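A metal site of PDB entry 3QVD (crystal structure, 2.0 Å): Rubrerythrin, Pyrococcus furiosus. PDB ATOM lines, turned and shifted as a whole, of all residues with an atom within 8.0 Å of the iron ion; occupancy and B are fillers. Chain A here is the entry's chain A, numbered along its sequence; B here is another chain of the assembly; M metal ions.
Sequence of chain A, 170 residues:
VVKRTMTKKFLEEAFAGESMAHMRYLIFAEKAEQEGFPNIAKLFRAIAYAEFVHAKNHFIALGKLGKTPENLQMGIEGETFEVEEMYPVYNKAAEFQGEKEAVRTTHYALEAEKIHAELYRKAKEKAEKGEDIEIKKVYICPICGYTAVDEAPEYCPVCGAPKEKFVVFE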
ATOM      1  N   TYR A 108       6.607  -4.957  -0.417  1.00  0.00           N
ATOM      2  CA  TYR A 108       6.895  -6.385  -0.420  1.00  0.00           C
ATOM      3  C   TYR A 108       6.150  -7.086  -1.558  1.00  0.00           C
ATOM      4  O   TYR A 108       6.753  -7.799  -2.363  1.00  0.00           O
ATOM      5  CB  TYR A 108       6.466  -7.032   0.910  1.00  0.00           C
ATOM      6  CG  TYR A 108       7.425  -6.852   2.072  1.00  0.00           C
ATOM      7  CD1 TYR A 108       8.637  -6.171   1.909  1.00  0.00           C
ATOM      8  CD2 TYR A 108       7.146  -7.389   3.329  1.00  0.00           C
ATOM      9  CE1 TYR A 108       9.542  -6.036   2.961  1.00  0.00           C
ATOM     10  CE2 TYR A 108       8.042  -7.257   4.391  1.00  0.00           C
ATOM     11  CZ  TYR A 108       9.238  -6.588   4.198  1.00  0.00           C
ATOM     12  OH  TYR A 108      10.136  -6.459   5.240  1.00  0.00           O
ATOM     13  N   ILE A 140      10.134 -19.581  -1.905  1.00  0.00           N
ATOM     14  CA  ILE A 140       9.270 -18.454  -1.590  1.00  0.00           C
ATOM     15  C   ILE A 140       9.665 -17.944  -0.214  1.00  0.00           C
ATOM     16  O   ILE A 140       9.751 -18.730   0.738  1.00  0.00           O
ATOM     17  CB  ILE A 140       7.763 -18.842  -1.527  1.00  0.00           C
ATOM     18  CG1 ILE A 140       7.327 -19.584  -2.793  1.00  0.00           C
ATOM     19  CG2 ILE A 140       6.924 -17.565  -1.363  1.00  0.00           C
ATOM     20  CD1 ILE A 140       7.319 -18.755  -4.058  1.00  0.00           C
ATOM     21  N   CYS A 141       9.907 -16.647  -0.101  1.00  0.00           N
ATOM     22  CA  CYS A 141      10.263 -16.070   1.190  1.00  0.00           C
ATOM     23  C   CYS A 141       8.983 -15.924   2.020  1.00  0.00           C
ATOM     24  O   CYS A 141       8.027 -15.289   1.585  1.00  0.00           O
ATOM     25  CB  CYS A 141      10.935 -14.706   0.980  1.00  0.00           C
ATOM     26  SG  CYS A 141      11.344 -13.828   2.507  1.00  0.00           S
ATOM     27  N   PRO A 142       8.969 -16.507   3.228  1.00  0.00           N
ATOM     28  CA  PRO A 142       7.803 -16.445   4.112  1.00  0.00           C
ATOM     29  C   PRO A 142       7.550 -15.061   4.692  1.00  0.00           C
ATOM     30  O   PRO A 142       6.504 -14.807   5.296  1.00  0.00           O
ATOM     31  CB  PRO A 142       8.134 -17.463   5.191  1.00  0.00           C
ATOM     32  CG  PRO A 142       9.613 -17.294   5.340  1.00  0.00           C
ATOM     33  CD  PRO A 142      10.075 -17.244   3.886  1.00  0.00           C
ATOM     34  N   ILE A 143       8.494 -14.151   4.491  1.00  0.00           N
ATOM     35  CA  ILE A 143       8.369 -12.800   5.007  1.00  0.00           C
ATOM     36  C   ILE A 143       7.745 -11.819   4.016  1.00  0.00           C
ATOM     37  O   ILE A 143       6.802 -11.100   4.361  1.00  0.00           O
ATOM     38  CB  ILE A 143       9.750 -12.242   5.447  1.00  0.00           C
ATOM     39  CG1 ILE A 143      10.386 -13.178   6.473  1.00  0.00           C
ATOM     40  CG2 ILE A 143       9.604 -10.851   6.046  1.00  0.00           C
ATOM     41  CD1 ILE A 143       9.513 -13.469   7.678  1.00  0.00           C
ATOM     42  N   CYS A 144       8.246 -11.798   2.793  1.00  0.00           N
ATOM     43  CA  CYS A 144       7.766 -10.867   1.783  1.00  0.00           C
ATOM     44  C   CYS A 144       7.217 -11.505   0.512  1.00  0.00           C
ATOM     45  O   CYS A 144       6.750 -10.802  -0.384  1.00  0.00           O
ATOM     46  CB  CYS A 144       8.906  -9.915   1.392  1.00  0.00           C
ATOM     47  SG  CYS A 144      10.198 -10.755   0.448  1.00  0.00           S
ATOM     48  N   GLY A 145       7.284 -12.827   0.412  1.00  0.00           N
ATOM     49  CA  GLY A 145       6.770 -13.500  -0.769  1.00  0.00           C
ATOM     50  C   GLY A 145       7.721 -13.504  -1.956  1.00  0.00           C
ATOM     51  O   GLY A 145       7.332 -13.926  -3.049  1.00  0.00           O
ATOM     52  N   TYR A 146       8.945 -13.018  -1.765  1.00  0.00           N
ATOM     53  CA  TYR A 146       9.918 -13.028  -2.857  1.00  0.00           C
ATOM     54  C   TYR A 146       9.931 -14.442  -3.436  1.00  0.00           C
ATOM     55  O   TYR A 146       9.895 -15.429  -2.680  1.00  0.00           O
ATOM     56  CB  TYR A 146      11.319 -12.639  -2.352  1.00  0.00           C
ATOM     57  CG  TYR A 146      12.441 -13.010  -3.297  1.00  0.00           C
ATOM     58  CD1 TYR A 146      13.176 -14.180  -3.111  1.00  0.00           C
ATOM     59  CD2 TYR A 146      12.757 -12.204  -4.396  1.00  0.00           C
ATOM     60  CE1 TYR A 146      14.201 -14.536  -3.976  1.00  0.00           C
ATOM     61  CE2 TYR A 146      13.788 -12.549  -5.272  1.00  0.00           C
ATOM     62  CZ  TYR A 146      14.501 -13.721  -5.047  1.00  0.00           C
ATOM     63  OH  TYR A 146      15.516 -14.080  -5.903  1.00  0.00           O
ATOM     64  N   THR A 147       9.998 -14.545  -4.754  1.00  0.00           N
ATOM     65  CA  THR A 147       9.945 -15.830  -5.439  1.00  0.00           C
ATOM     66  C   THR A 147      11.155 -16.085  -6.332  1.00  0.00           C
ATOM     67  O   THR A 147      11.590 -15.203  -7.065  1.00  0.00           O
ATOM     68  CB  THR A 147       8.660 -15.896  -6.284  1.00  0.00           C
ATOM     69  OG1 THR A 147       7.521 -15.650  -5.434  1.00  0.00           O
ATOM     70  CG2 THR A 147       8.504 -17.246  -6.949  1.00  0.00           C
ATOM     71  N   TYR A 155      20.427 -14.486   0.390  1.00  0.00           N
ATOM     72  CA  TYR A 155      19.562 -13.682   1.248  1.00  0.00           C
ATOM     73  C   TYR A 155      18.479 -13.054   0.364  1.00  0.00           C
ATOM     74  O   TYR A 155      18.759 -12.673  -0.779  1.00  0.00           O
ATOM     75  CB  TYR A 155      20.382 -12.586   1.932  1.00  0.00           C
ATOM     76  CG  TYR A 155      21.404 -13.112   2.916  1.00  0.00           C
ATOM     77  CD1 TYR A 155      21.024 -13.549   4.180  1.00  0.00           C
ATOM     78  CD2 TYR A 155      22.758 -13.214   2.564  1.00  0.00           C
ATOM     79  CE1 TYR A 155      21.948 -14.093   5.066  1.00  0.00           C
ATOM     80  CE2 TYR A 155      23.691 -13.753   3.451  1.00  0.00           C
ATOM     81  CZ  TYR A 155      23.277 -14.186   4.700  1.00  0.00           C
ATOM     82  OH  TYR A 155      24.201 -14.731   5.577  1.00  0.00           O
ATOM     83  N   CYS A 156      17.260 -12.971   0.885  1.00  0.00           N
ATOM     84  CA  CYS A 156      16.160 -12.361   0.124  1.00  0.00           C
ATOM     85  C   CYS A 156      16.537 -10.921  -0.217  1.00  0.00           C
ATOM     86  O   CYS A 156      16.878 -10.137   0.668  1.00  0.00           O
ATOM     87  CB  CYS A 156      14.867 -12.379   0.946  1.00  0.00           C
ATOM     88  SG  CYS A 156      13.490 -11.541   0.106  1.00  0.00           S
ATOM     89  N   PRO A 157      16.458 -10.538  -1.497  1.00  0.00           N
ATOM     90  CA  PRO A 157      16.805  -9.171  -1.922  1.00  0.00           C
ATOM     91  C   PRO A 157      15.830  -8.099  -1.457  1.00  0.00           C
ATOM     92  O   PRO A 157      16.145  -6.902  -1.516  1.00  0.00           O
ATOM     93  CB  PRO A 157      16.842  -9.292  -3.443  1.00  0.00           C
ATOM     94  CG  PRO A 157      15.769 -10.294  -3.728  1.00  0.00           C
ATOM     95  CD  PRO A 157      16.007 -11.353  -2.642  1.00  0.00           C
ATOM     96  N   VAL A 158      14.660  -8.506  -0.995  1.00  0.00           N
ATOM     97  CA  VAL A 158      13.669  -7.543  -0.537  1.00  0.00           C
ATOM     98  C   VAL A 158      13.719  -7.298   0.965  1.00  0.00           C
ATOM     99  O   VAL A 158      13.807  -6.144   1.398  1.00  0.00           O
ATOM    100  CB  VAL A 158      12.233  -7.983  -0.927  1.00  0.00           C
ATOM    101  CG1 VAL A 158      11.218  -6.948  -0.441  1.00  0.00           C
ATOM    102  CG2 VAL A 158      12.122  -8.168  -2.433  1.00  0.00           C
ATOM    103  N   CYS A 159      13.685  -8.366   1.763  1.00  0.00           N
ATOM    104  CA  CYS A 159      13.719  -8.226   3.218  1.00  0.00           C
ATOM    105  C   CYS A 159      15.018  -8.711   3.868  1.00  0.00           C
ATOM    106  O   CYS A 159      15.248  -8.477   5.054  1.00  0.00           O
ATOM    107  CB  CYS A 159      12.539  -8.962   3.848  1.00  0.00           C
ATOM    108  SG  CYS A 159      12.605 -10.765   3.735  1.00  0.00           S
ATOM    109  N   GLY A 160      15.847  -9.416   3.094  1.00  0.00           N
ATOM    110  CA  GLY A 160      17.110  -9.884   3.627  1.00  0.00           C
ATOM    111  C   GLY A 160      17.091 -11.178   4.428  1.00  0.00           C
ATOM    112  O   GLY A 160      18.098 -11.549   5.024  1.00  0.00           O
ATOM    113  N   ALA A 161      15.952 -11.865   4.447  1.00  0.00           N
ATOM    114  CA  ALA A 161      15.843 -13.124   5.174  1.00  0.00           C
ATOM    115  C   ALA A 161      16.801 -14.149   4.579  1.00  0.00           C
ATOM    116  O   ALA A 161      16.998 -14.186   3.366  1.00  0.00           O
ATOM    117  CB  ALA A 161      14.409 -13.640   5.089  1.00  0.00           C
ATOM    118  N   PRO A 162      17.417 -14.983   5.427  1.00  0.00           N
ATOM    119  CA  PRO A 162      18.353 -15.990   4.920  1.00  0.00           C
ATOM    120  C   PRO A 162      17.643 -17.080   4.123  1.00  0.00           C
ATOM    121  O   PRO A 162      16.493 -17.422   4.406  1.00  0.00           O
ATOM    122  CB  PRO A 162      19.017 -16.523   6.195  1.00  0.00           C
ATOM    123  CG  PRO A 162      17.926 -16.392   7.208  1.00  0.00           C
ATOM    124  CD  PRO A 162      17.366 -15.020   6.909  1.00  0.00           C
ATOM    125  N   PHE A 166      13.465 -19.874   3.378  1.00  0.00           N
ATOM    126  CA  PHE A 166      12.596 -19.960   2.201  1.00  0.00           C
ATOM    127  C   PHE A 166      11.782 -21.262   2.186  1.00  0.00           C
ATOM    128  O   PHE A 166      12.307 -22.340   2.481  1.00  0.00           O
ATOM    129  CB  PHE A 166      13.408 -19.892   0.900  1.00  0.00           C
ATOM    130  CG  PHE A 166      14.141 -18.591   0.684  1.00  0.00           C
ATOM    131  CD1 PHE A 166      13.963 -17.510   1.548  1.00  0.00           C
ATOM    132  CD2 PHE A 166      14.997 -18.441  -0.402  1.00  0.00           C
ATOM    133  CE1 PHE A 166      14.637 -16.294   1.318  1.00  0.00           C
ATOM    134  CE2 PHE A 166      15.671 -17.248  -0.639  1.00  0.00           C
ATOM    135  CZ  PHE A 166      15.485 -16.173   0.215  1.00  0.00           C
ATOM    136  N   VAL B  53       1.447 -15.068   1.752  1.00  0.00           N
ATOM    137  CA  VAL B  53       2.352 -14.237   2.543  1.00  0.00           C
ATOM    138  C   VAL B  53       1.912 -12.779   2.415  1.00  0.00           C
ATOM    139  O   VAL B  53       1.798 -12.066   3.419  1.00  0.00           O
ATOM    140  CB  VAL B  53       3.805 -14.377   2.043  1.00  0.00           C
ATOM    141  CG1 VAL B  53       4.693 -13.359   2.745  1.00  0.00           C
ATOM    142  CG2 VAL B  53       4.316 -15.786   2.323  1.00  0.00           C
HETATM  143 FE    FE M   1      11.900 -11.709   1.732  1.00  0.00          FE
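Within 4 Å of the iron ion: Cys 141, Cys 144, Cys 156 and Cys 159.
The iron ion is bound by SG of Cys 156 (2.3 Å), SG of Cys 141 (2.3 Å), SG of Cys 159 (2.3 Å) and SG of Cys 144 (2.3 Å).
The backbone NH of Cys 156 sits at hydrogen-bond distance from the backbone carbonyl oxygen of Ala 161 (2.8 Å). N of Ala 161 sits close to SG of Cys 159. N of Ile 143 sits close to SG of Cys 141. The side-chain sulfur (SG) of Cys 156 sits close to the backbone NH (N) of Val 158 (3.4 Å). The backbone NH (N) of Cys 141 lies within hydrogen-bond range of the backbone carbonyl oxygen (O) of Tyr 146 (2.9 Å). SG of Cys 144 lies close to N of Tyr 146, 3.4 Å away.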
